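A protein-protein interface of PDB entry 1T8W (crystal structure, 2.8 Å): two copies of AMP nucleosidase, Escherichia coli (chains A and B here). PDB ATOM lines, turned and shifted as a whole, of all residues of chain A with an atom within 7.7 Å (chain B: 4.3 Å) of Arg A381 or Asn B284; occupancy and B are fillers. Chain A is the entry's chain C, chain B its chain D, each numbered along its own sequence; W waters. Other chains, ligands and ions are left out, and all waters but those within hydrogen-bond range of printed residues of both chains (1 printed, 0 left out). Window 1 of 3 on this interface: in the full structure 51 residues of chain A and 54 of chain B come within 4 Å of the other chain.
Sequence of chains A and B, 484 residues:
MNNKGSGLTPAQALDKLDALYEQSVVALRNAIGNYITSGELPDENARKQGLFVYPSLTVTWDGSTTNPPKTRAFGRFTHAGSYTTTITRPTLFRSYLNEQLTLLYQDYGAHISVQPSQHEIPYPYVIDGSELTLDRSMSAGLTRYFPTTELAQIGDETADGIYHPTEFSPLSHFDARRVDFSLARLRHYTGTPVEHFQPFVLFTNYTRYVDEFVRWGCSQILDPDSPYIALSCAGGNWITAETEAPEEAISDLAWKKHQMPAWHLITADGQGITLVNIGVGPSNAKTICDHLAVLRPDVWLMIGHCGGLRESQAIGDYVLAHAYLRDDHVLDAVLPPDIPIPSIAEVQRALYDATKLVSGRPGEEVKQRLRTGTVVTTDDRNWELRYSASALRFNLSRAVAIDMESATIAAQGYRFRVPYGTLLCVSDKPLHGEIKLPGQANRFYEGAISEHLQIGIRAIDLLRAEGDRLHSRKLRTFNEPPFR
The backbone carbonyl oxygen (O) of Asp A379 is in hydrogen-bond range of the side-chain hydroxyl (OG) of Ser B283, 2.7 Å away. NH1 of Arg A381 is in hydrogen-bond range of OE1 of Gln B259. The side-chain carboxylate (OD1) of Asp A380 is in salt-bridge range of the side-chain amino group (NZ) of Lys B286. ND2 of Asn B284 sits close to NH2 of Arg A381 (2.8 Å).
The side-chain carboxylate (OD1) of Asp A380 sits close to the backbone NH (N) of Asn A382. The side-chain hydroxyl of Thr A378 is in hydrogen-bond range of the backbone NH of Asp A380, at 3.0 Å. The side-chain amide oxygen (OD1) of Asn B284 lies close to the backbone carbonyl oxygen (O) of Ile B278 (3.1 Å). O of Ser B283 is in hydrogen-bond range of OG1 of Thr B287 (2.8 Å). O of Tyr B189 is in hydrogen-bond range of N of Met B260.
Among the printed residues, pairs that only touch across the chains: Arg A381 with Tyr B189, Arg A381 with Thr B287, Val A280 with Gln B259, Asn A382 with Thr B287 and Arg A381 with Met B260.
Asn A284 touches none of the printed residues of chain B. Of chain B, only Tyr B189, Gln B259, Met B260, Asn B284 and Thr B287 come within 4 Å of Arg A381. Of the printed residues of chain A, Gln B259 touches Val A280 and Arg A381. Printed residues of chain A within 4 Å of Ser B283: Asp A379 (2.7 Å). Of the printed residues of chain A, Lys B286 touches Asp A380. The nearest printed residue of chain B that does not touch Arg A381 is Ser B283 (5.3 Å). The nearest residue of chain A that does not touch Asn B284 is Val A280 (4.9 Å). The nearest printed residue of chain A that does not touch Tyr B189 is Asn A382 (4.9 Å).
Of the 12 printed residues of chain B, 7 touch a printed residue of chain A. Hydrophobic or aromatic side chains of chain B that line the printed part of chain A: Tyr B189 and Met B260. Along chain B the printed residues that touch a printed residue of chain A span positions 189 to 287. Of the 21 printed residues of chain A, 5 touch a printed residue of chain B. Hydrophobic or aromatic side chains of chain A that line the printed part of chain B: Val A280. Among the printed residues, Asp or Glu carboxylates within 4 Å of a Lys or Arg side-chain nitrogen of the other chain: Asp A380 with Lys B286 (2.8 Å).
Positions printed for both chains: 281, 282, 283 and 284. Of the 9 pairs that touch across the chains among the printed residues, none has its exchanged pair printed and touching as well.
Water W1 bridges the guanidinium group (NH1) of Arg A381 and the side-chain hydroxyl (OH) of Tyr B189.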
ATOM      1  N   ASN A 205      15.630 -10.358   7.934  1.00  0.00           N
ATOM      2  CA  ASN A 205      16.294 -11.497   8.556  1.00  0.00           C
ATOM      3  C   ASN A 205      16.073 -11.492  10.055  1.00  0.00           C
ATOM      4  O   ASN A 205      16.830 -12.091  10.807  1.00  0.00           O
ATOM      5  CB  ASN A 205      17.804 -11.471   8.269  1.00  0.00           C
ATOM      6  CG  ASN A 205      18.462 -10.145   8.634  1.00  0.00           C
ATOM      7  OD1 ASN A 205      17.956  -9.385   9.437  1.00  0.00           O
ATOM      8  ND2 ASN A 205      19.610  -9.879   8.047  1.00  0.00           N
ATOM      9  N   GLY A 279      14.565 -15.284   6.945  1.00  0.00           N
ATOM     10  CA  GLY A 279      15.365 -15.936   7.950  1.00  0.00           C
ATOM     11  C   GLY A 279      16.798 -15.528   7.760  1.00  0.00           C
ATOM     12  O   GLY A 279      17.063 -14.431   7.270  1.00  0.00           O
ATOM     13  N   VAL A 280      17.723 -16.409   8.125  1.00  0.00           N
ATOM     14  CA  VAL A 280      19.134 -16.098   8.006  1.00  0.00           C
ATOM     15  C   VAL A 280      19.796 -17.158   7.130  1.00  0.00           C
ATOM     16  O   VAL A 280      19.342 -18.309   7.091  1.00  0.00           O
ATOM     17  CB  VAL A 280      19.794 -16.027   9.430  1.00  0.00           C
ATOM     18  CG1 VAL A 280      20.344 -17.391   9.828  1.00  0.00           C
ATOM     19  CG2 VAL A 280      20.877 -14.958   9.465  1.00  0.00           C
ATOM     20  N   GLY A 281      20.844 -16.756   6.405  1.00  0.00           N
ATOM     21  CA  GLY A 281      21.552 -17.688   5.543  1.00  0.00           C
ATOM     22  C   GLY A 281      21.386 -17.436   4.051  1.00  0.00           C
ATOM     23  O   GLY A 281      20.344 -16.938   3.614  1.00  0.00           O
ATOM     24  N   PRO A 282      22.409 -17.756   3.237  1.00  0.00           N
ATOM     25  CA  PRO A 282      22.336 -17.548   1.793  1.00  0.00           C
ATOM     26  C   PRO A 282      21.399 -18.545   1.105  1.00  0.00           C
ATOM     27  O   PRO A 282      20.768 -18.213   0.109  1.00  0.00           O
ATOM     28  CB  PRO A 282      23.789 -17.716   1.359  1.00  0.00           C
ATOM     29  CG  PRO A 282      24.538 -17.308   2.555  1.00  0.00           C
ATOM     30  CD  PRO A 282      23.802 -18.006   3.630  1.00  0.00           C
ATOM     31  N   SER A 283      21.311 -19.758   1.644  1.00  0.00           N
ATOM     32  CA  SER A 283      20.445 -20.789   1.075  1.00  0.00           C
ATOM     33  C   SER A 283      19.012 -20.311   0.950  1.00  0.00           C
ATOM     34  O   SER A 283      18.385 -20.479  -0.085  1.00  0.00           O
ATOM     35  CB  SER A 283      20.448 -22.061   1.934  1.00  0.00           C
ATOM     36  OG  SER A 283      21.621 -22.826   1.751  1.00  0.00           O
ATOM     37  N   ASN A 284      18.478 -19.728   2.007  1.00  0.00           N
ATOM     38  CA  ASN A 284      17.116 -19.256   1.940  1.00  0.00           C
ATOM     39  C   ASN A 284      16.981 -18.084   0.998  1.00  0.00           C
ATOM     40  O   ASN A 284      16.031 -18.029   0.212  1.00  0.00           O
ATOM     41  CB  ASN A 284      16.634 -18.850   3.314  1.00  0.00           C
ATOM     42  CG  ASN A 284      16.247 -20.025   4.148  1.00  0.00           C
ATOM     43  OD1 ASN A 284      15.662 -19.858   5.216  1.00  0.00           O
ATOM     44  ND2 ASN A 284      16.565 -21.231   3.674  1.00  0.00           N
ATOM     45  N   HIS A 305      19.658  -6.760   9.647  1.00  0.00           N
ATOM     46  CA  HIS A 305      20.763  -6.376  10.514  1.00  0.00           C
ATOM     47  C   HIS A 305      22.066  -6.900   9.935  1.00  0.00           C
ATOM     48  O   HIS A 305      22.072  -7.791   9.080  1.00  0.00           O
ATOM     49  CB  HIS A 305      20.559  -6.945  11.925  1.00  0.00           C
ATOM     50  CG  HIS A 305      20.479  -8.440  11.968  1.00  0.00           C
ATOM     51  ND1 HIS A 305      21.589  -9.249  11.870  1.00  0.00           N
ATOM     52  CD2 HIS A 305      19.415  -9.274  12.041  1.00  0.00           C
ATOM     53  CE1 HIS A 305      21.213 -10.515  11.875  1.00  0.00           C
ATOM     54  NE2 HIS A 305      19.898 -10.558  11.978  1.00  0.00           N
ATOM     55  N   THR A 378      28.370 -13.761   3.895  1.00  0.00           N
ATOM     56  CA  THR A 378      28.984 -15.063   4.149  1.00  0.00           C
ATOM     57  C   THR A 378      27.979 -16.147   4.480  1.00  0.00           C
ATOM     58  O   THR A 378      26.855 -15.871   4.903  1.00  0.00           O
ATOM     59  CB  THR A 378      29.968 -14.975   5.333  1.00  0.00           C
ATOM     60  OG1 THR A 378      30.568 -16.250   5.561  1.00  0.00           O
ATOM     61  CG2 THR A 378      29.238 -14.538   6.601  1.00  0.00           C
ATOM     62  N   ASP A 379      28.398 -17.389   4.298  1.00  0.00           N
ATOM     63  CA  ASP A 379      27.537 -18.518   4.613  1.00  0.00           C
ATOM     64  C   ASP A 379      28.002 -19.185   5.893  1.00  0.00           C
ATOM     65  O   ASP A 379      27.498 -20.244   6.260  1.00  0.00           O
ATOM     66  CB  ASP A 379      27.511 -19.528   3.452  1.00  0.00           C
ATOM     67  CG  ASP A 379      28.835 -20.274   3.253  1.00  0.00           C
ATOM     68  OD1 ASP A 379      29.905 -19.805   3.688  1.00  0.00           O
ATOM     69  OD2 ASP A 379      28.804 -21.347   2.624  1.00  0.00           O
ATOM     70  N   ASP A 380      28.959 -18.546   6.569  1.00  0.00           N
ATOM     71  CA  ASP A 380      29.523 -19.054   7.815  1.00  0.00           C
ATOM     72  C   ASP A 380      29.111 -18.195   8.994  1.00  0.00           C
ATOM     73  O   ASP A 380      29.708 -17.168   9.279  1.00  0.00           O
ATOM     74  CB  ASP A 380      31.036 -19.085   7.727  1.00  0.00           C
ATOM     75  CG  ASP A 380      31.674 -19.781   8.904  1.00  0.00           C
ATOM     76  OD1 ASP A 380      30.949 -20.332   9.758  1.00  0.00           O
ATOM     77  OD2 ASP A 380      32.915 -19.785   8.969  1.00  0.00           O
ATOM     78  N   ARG A 381      28.086 -18.638   9.697  1.00  0.00           N
ATOM     79  CA  ARG A 381      27.583 -17.895  10.826  1.00  0.00           C
ATOM     80  C   ARG A 381      28.661 -17.630  11.864  1.00  0.00           C
ATOM     81  O   ARG A 381      28.640 -16.600  12.541  1.00  0.00           O
ATOM     82  CB  ARG A 381      26.428 -18.638  11.457  1.00  0.00           C
ATOM     83  CG  ARG A 381      25.882 -17.908  12.634  1.00  0.00           C
ATOM     84  CD  ARG A 381      24.432 -17.530  12.421  1.00  0.00           C
ATOM     85  NE  ARG A 381      23.630 -18.697  12.067  1.00  0.00           N
ATOM     86  CZ  ARG A 381      22.315 -18.752  12.224  1.00  0.00           C
ATOM     87  NH1 ARG A 381      21.677 -17.703  12.731  1.00  0.00           N
ATOM     88  NH2 ARG A 381      21.643 -19.845  11.871  1.00  0.00           N
ATOM     89  N   ASN A 382      29.610 -18.555  11.991  1.00  0.00           N
ATOM     90  CA  ASN A 382      30.686 -18.386  12.950  1.00  0.00           C
ATOM     91  C   ASN A 382      31.978 -17.946  12.307  1.00  0.00           C
ATOM     92  O   ASN A 382      33.045 -18.384  12.692  1.00  0.00           O
ATOM     93  CB  ASN A 382      30.928 -19.665  13.730  1.00  0.00           C
ATOM     94  CG  ASN A 382      29.780 -20.025  14.598  1.00  0.00           C
ATOM     95  OD1 ASN A 382      29.161 -19.161  15.225  1.00  0.00           O
ATOM     96  ND2 ASN A 382      29.483 -21.311  14.662  1.00  0.00           N
ATOM     97  N   TRP A 383      31.880 -17.061  11.330  1.00  0.00           N
ATOM     98  CA  TRP A 383      33.059 -16.562  10.642  1.00  0.00           C
ATOM     99  C   TRP A 383      34.061 -15.973  11.632  1.00  0.00           C
ATOM    100  O   TRP A 383      35.262 -15.996  11.397  1.00  0.00           O
ATOM    101  CB  TRP A 383      32.651 -15.504   9.610  1.00  0.00           C
ATOM    102  CG  TRP A 383      31.972 -14.322  10.208  1.00  0.00           C
ATOM    103  CD1 TRP A 383      30.640 -14.169  10.433  1.00  0.00           C
ATOM    104  CD2 TRP A 383      32.604 -13.152  10.726  1.00  0.00           C
ATOM    105  NE1 TRP A 383      30.398 -12.971  11.061  1.00  0.00           N
ATOM    106  CE2 TRP A 383      31.587 -12.326  11.253  1.00  0.00           C
ATOM    107  CE3 TRP A 383      33.931 -12.721  10.797  1.00  0.00           C
ATOM    108  CZ2 TRP A 383      31.853 -11.095  11.844  1.00  0.00           C
ATOM    109  CZ3 TRP A 383      34.198 -11.496  11.383  1.00  0.00           C
ATOM    110  CH2 TRP A 383      33.158 -10.695  11.901  1.00  0.00           C
ATOM    111  N   GLU A 384      33.564 -15.448  12.747  1.00  0.00           N
ATOM    112  CA  GLU A 384      34.441 -14.869  13.754  1.00  0.00           C
ATOM    113  C   GLU A 384      35.525 -15.867  14.191  1.00  0.00           C
ATOM    114  O   GLU A 384      36.637 -15.482  14.509  1.00  0.00           O
ATOM    115  CB  GLU A 384      33.620 -14.428  14.969  1.00  0.00           C
ATOM    116  CG  GLU A 384      32.553 -13.396  14.659  1.00  0.00           C
ATOM    117  CD  GLU A 384      31.123 -13.965  14.644  1.00  0.00           C
ATOM    118  OE1 GLU A 384      30.919 -15.109  14.160  1.00  0.00           O
ATOM    119  OE2 GLU A 384      30.197 -13.242  15.104  1.00  0.00           O
ATOM    120  N   LEU A 385      35.198 -17.155  14.206  1.00  0.00           N
ATOM    121  CA  LEU A 385      36.168 -18.155  14.614  1.00  0.00           C
ATOM    122  C   LEU A 385      37.299 -18.271  13.621  1.00  0.00           C
ATOM    123  O   LEU A 385      38.267 -18.968  13.866  1.00  0.00           O
ATOM    124  CB  LEU A 385      35.510 -19.518  14.768  1.00  0.00           C
ATOM    125  CG  LEU A 385      34.493 -19.666  15.887  1.00  0.00           C
ATOM    126  CD1 LEU A 385      33.981 -21.096  15.878  1.00  0.00           C
ATOM    127  CD2 LEU A 385      35.107 -19.296  17.212  1.00  0.00           C
ATOM    128  N   ILE A 402      29.147  -6.860   7.465  1.00  0.00           N
ATOM    129  CA  ILE A 402      29.054  -8.265   7.107  1.00  0.00           C
ATOM    130  C   ILE A 402      27.663  -8.819   7.448  1.00  0.00           C
ATOM    131  O   ILE A 402      27.118  -8.560   8.515  1.00  0.00           O
ATOM    132  CB  ILE A 402      30.141  -9.088   7.816  1.00  0.00           C
ATOM    133  CG1 ILE A 402      30.025 -10.557   7.413  1.00  0.00           C
ATOM    134  CG2 ILE A 402      30.039  -8.905   9.313  1.00  0.00           C
ATOM    135  CD1 ILE A 402      31.169 -11.376   7.851  1.00  0.00           C
ATOM    136  N   MET A 404      24.508 -12.046   5.915  1.00  0.00           N
ATOM    137  CA  MET A 404      24.407 -13.361   5.315  1.00  0.00           C
ATOM    138  C   MET A 404      23.338 -13.523   4.247  1.00  0.00           C
ATOM    139  O   MET A 404      23.010 -14.647   3.880  1.00  0.00           O
ATOM    140  CB  MET A 404      24.192 -14.398   6.400  1.00  0.00           C
ATOM    141  CG  MET A 404      25.323 -14.459   7.400  1.00  0.00           C
ATOM    142  SD  MET A 404      25.050 -15.834   8.763  1.00  0.00           S
ATOM    143  CE  MET A 404      25.294 -17.434   7.678  1.00  0.00           C
ATOM    144  N   GLU A 405      22.814 -12.416   3.726  1.00  0.00           N
ATOM    145  CA  GLU A 405      21.767 -12.490   2.718  1.00  0.00           C
ATOM    146  C   GLU A 405      21.955 -11.525   1.552  1.00  0.00           C
ATOM    147  O   GLU A 405      21.690 -11.886   0.408  1.00  0.00           O
ATOM    148  CB  GLU A 405      20.402 -12.236   3.361  1.00  0.00           C
ATOM    149  CG  GLU A 405      19.962 -13.237   4.422  1.00  0.00           C
ATOM    150  CD  GLU A 405      20.537 -12.948   5.807  1.00  0.00           C
ATOM    151  OE1 GLU A 405      20.818 -11.765   6.105  1.00  0.00           O
ATOM    152  OE2 GLU A 405      20.691 -13.907   6.598  1.00  0.00           O
ATOM    153  N   LEU A 437      23.908 -10.722  19.756  1.00  0.00           N
ATOM    154  CA  LEU A 437      23.107 -11.605  18.894  1.00  0.00           C
ATOM    155  C   LEU A 437      21.651 -11.163  18.746  1.00  0.00           C
ATOM    156  O   LEU A 437      21.068 -10.569  19.663  1.00  0.00           O
ATOM    157  CB  LEU A 437      23.112 -13.033  19.429  1.00  0.00           C
ATOM    158  CG  LEU A 437      24.346 -13.888  19.164  1.00  0.00           C
ATOM    159  CD1 LEU A 437      25.620 -13.150  19.552  1.00  0.00           C
ATOM    160  CD2 LEU A 437      24.206 -15.168  19.958  1.00  0.00           C
ATOM    161  N   PRO A 438      21.043 -11.435  17.575  1.00  0.00           N
ATOM    162  CA  PRO A 438      19.645 -11.045  17.370  1.00  0.00           C
ATOM    163  C   PRO A 438      18.737 -11.809  18.339  1.00  0.00           C
ATOM    164  O   PRO A 438      18.562 -13.026  18.235  1.00  0.00           O
ATOM    165  CB  PRO A 438      19.410 -11.395  15.905  1.00  0.00           C
ATOM    166  CG  PRO A 438      20.749 -11.093  15.306  1.00  0.00           C
ATOM    167  CD  PRO A 438      21.670 -11.775  16.286  1.00  0.00           C
ATOM    168  N   TYR B 189      20.638 -20.185  20.525  1.00  0.00           N
ATOM    169  CA  TYR B 189      20.082 -20.929  19.402  1.00  0.00           C
ATOM    170  C   TYR B 189      19.108 -22.008  19.802  1.00  0.00           C
ATOM    171  O   TYR B 189      18.140 -22.304  19.100  1.00  0.00           O
ATOM    172  CB  TYR B 189      21.192 -21.601  18.600  1.00  0.00           C
ATOM    173  CG  TYR B 189      22.038 -20.664  17.798  1.00  0.00           C
ATOM    174  CD1 TYR B 189      21.457 -19.735  16.948  1.00  0.00           C
ATOM    175  CD2 TYR B 189      23.424 -20.722  17.859  1.00  0.00           C
ATOM    176  CE1 TYR B 189      22.234 -18.886  16.179  1.00  0.00           C
ATOM    177  CE2 TYR B 189      24.210 -19.879  17.091  1.00  0.00           C
ATOM    178  CZ  TYR B 189      23.607 -18.962  16.257  1.00  0.00           C
ATOM    179  OH  TYR B 189      24.364 -18.093  15.511  1.00  0.00           O
ATOM    180  N   GLN B 259      16.291 -20.385  16.516  1.00  0.00           N
ATOM    181  CA  GLN B 259      16.576 -20.924  15.202  1.00  0.00           C
ATOM    182  C   GLN B 259      16.771 -22.418  15.196  1.00  0.00           C
ATOM    183  O   GLN B 259      16.493 -23.070  14.194  1.00  0.00           O
ATOM    184  CB  GLN B 259      17.806 -20.248  14.627  1.00  0.00           C
ATOM    185  CG  GLN B 259      17.601 -18.772  14.392  1.00  0.00           C
ATOM    186  CD  GLN B 259      18.828 -18.122  13.803  1.00  0.00           C
ATOM    187  OE1 GLN B 259      19.351 -18.578  12.778  1.00  0.00           O
ATOM    188  NE2 GLN B 259      19.304 -17.049  14.446  1.00  0.00           N
ATOM    189  N   MET B 260      17.258 -22.962  16.304  1.00  0.00           N
ATOM    190  CA  MET B 260      17.477 -24.399  16.401  1.00  0.00           C
ATOM    191  C   MET B 260      17.075 -24.886  17.763  1.00  0.00           C
ATOM    192  O   MET B 260      17.911 -25.119  18.630  1.00  0.00           O
ATOM    193  CB  MET B 260      18.932 -24.731  16.130  1.00  0.00           C
ATOM    194  CG  MET B 260      19.307 -24.459  14.697  1.00  0.00           C
ATOM    195  SD  MET B 260      21.181 -24.178  14.461  1.00  0.00           S
ATOM    196  CE  MET B 260      21.243 -22.248  14.737  1.00  0.00           C
ATOM    197  N   ILE B 278      17.797 -28.739  13.821  1.00  0.00           N
ATOM    198  CA  ILE B 278      18.691 -27.797  13.182  1.00  0.00           C
ATOM    199  C   ILE B 278      18.114 -27.102  11.977  1.00  0.00           C
ATOM    200  O   ILE B 278      18.749 -26.226  11.390  1.00  0.00           O
ATOM    201  CB  ILE B 278      19.999 -28.466  12.798  1.00  0.00           C
ATOM    202  CG1 ILE B 278      19.763 -29.541  11.741  1.00  0.00           C
ATOM    203  CG2 ILE B 278      20.630 -29.033  14.033  1.00  0.00           C
ATOM    204  CD1 ILE B 278      20.996 -30.357  11.435  1.00  0.00           C
ATOM    205  N   GLY B 281      19.586 -26.801   5.760  1.00  0.00           N
ATOM    206  CA  GLY B 281      20.744 -26.068   5.274  1.00  0.00           C
ATOM    207  C   GLY B 281      22.069 -26.433   5.921  1.00  0.00           C
ATOM    208  O   GLY B 281      22.109 -26.842   7.082  1.00  0.00           O
ATOM    209  N   PRO B 282      23.180 -26.309   5.183  1.00  0.00           N
ATOM    210  CA  PRO B 282      24.493 -26.638   5.742  1.00  0.00           C
ATOM    211  C   PRO B 282      24.982 -25.592   6.752  1.00  0.00           C
ATOM    212  O   PRO B 282      25.701 -25.912   7.688  1.00  0.00           O
ATOM    213  CB  PRO B 282      25.381 -26.720   4.505  1.00  0.00           C
ATOM    214  CG  PRO B 282      24.417 -27.079   3.409  1.00  0.00           C
ATOM    215  CD  PRO B 282      23.255 -26.196   3.716  1.00  0.00           C
ATOM    216  N   SER B 283      24.582 -24.339   6.566  1.00  0.00           N
ATOM    217  CA  SER B 283      24.992 -23.276   7.482  1.00  0.00           C
ATOM    218  C   SER B 283      24.611 -23.624   8.891  1.00  0.00           C
ATOM    219  O   SER B 283      25.431 -23.556   9.798  1.00  0.00           O
ATOM    220  CB  SER B 283      24.337 -21.937   7.135  1.00  0.00           C
ATOM    221  OG  SER B 283      25.050 -21.271   6.108  1.00  0.00           O
ATOM    222  N   ASN B 284      23.353 -23.991   9.079  1.00  0.00           N
ATOM    223  CA  ASN B 284      22.895 -24.341  10.407  1.00  0.00           C
ATOM    224  C   ASN B 284      23.611 -25.557  10.940  1.00  0.00           C
ATOM    225  O   ASN B 284      24.119 -25.554  12.057  1.00  0.00           O
ATOM    226  CB  ASN B 284      21.394 -24.558  10.388  1.00  0.00           C
ATOM    227  CG  ASN B 284      20.635 -23.251  10.454  1.00  0.00           C
ATOM    228  OD1 ASN B 284      19.423 -23.233  10.679  1.00  0.00           O
ATOM    229  ND2 ASN B 284      21.351 -22.137  10.266  1.00  0.00           N
ATOM    230  N   ALA B 285      23.661 -26.599  10.128  1.00  0.00           N
ATOM    231  CA  ALA B 285      24.337 -27.808  10.519  1.00  0.00           C
ATOM    232  C   ALA B 285      25.738 -27.462  11.018  1.00  0.00           C
ATOM    233  O   ALA B 285      26.157 -27.933  12.071  1.00  0.00           O
ATOM    234  CB  ALA B 285      24.409 -28.770   9.336  1.00  0.00           C
ATOM    235  N   LYS B 286      26.457 -26.632  10.273  1.00  0.00           N
ATOM    236  CA  LYS B 286      27.792 -26.284  10.673  1.00  0.00           C
ATOM    237  C   LYS B 286      27.777 -25.535  11.974  1.00  0.00           C
ATOM    238  O   LYS B 286      28.460 -25.901  12.922  1.00  0.00           O
ATOM    239  CB  LYS B 286      28.485 -25.420   9.620  1.00  0.00           C
ATOM    240  CG  LYS B 286      29.888 -25.011  10.060  1.00  0.00           C
ATOM    241  CD  LYS B 286      30.549 -24.105   9.089  1.00  0.00           C
ATOM    242  CE  LYS B 286      31.874 -23.580   9.645  1.00  0.00           C
ATOM    243  NZ  LYS B 286      31.749 -22.724  10.859  1.00  0.00           N
ATOM    244  N   THR B 287      26.983 -24.476  12.010  1.00  0.00           N
ATOM    245  CA  THR B 287      26.884 -23.618  13.180  1.00  0.00           C
ATOM    246  C   THR B 287      26.548 -24.341  14.460  1.00  0.00           C
ATOM    247  O   THR B 287      27.188 -24.119  15.482  1.00  0.00           O
ATOM    248  CB  THR B 287      25.834 -22.517  12.978  1.00  0.00           C
ATOM    249  OG1 THR B 287      26.157 -21.766  11.810  1.00  0.00           O
ATOM    250  CG2 THR B 287      25.813 -21.559  14.179  1.00  0.00           C
ATOM    251  N   ILE B 288      25.538 -25.196  14.415  1.00  0.00           N
ATOM    252  CA  ILE B 288      25.147 -25.893  15.620  1.00  0.00           C
ATOM    253  C   ILE B 288      26.263 -26.788  16.138  1.00  0.00           C
ATOM    254  O   ILE B 288      26.509 -26.830  17.340  1.00  0.00           O
ATOM    255  CB  ILE B 288      23.853 -26.723  15.412  1.00  0.00           C
ATOM    256  CG1 ILE B 288      23.312 -27.140  16.775  1.00  0.00           C
ATOM    257  CG2 ILE B 288      24.105 -27.918  14.481  1.00  0.00           C
ATOM    258  CD1 ILE B 288      22.952 -25.943  17.614  1.00  0.00           C
HETATM  259  O   HOH W   1      22.737 -15.673  14.133  1.00  0.00           O
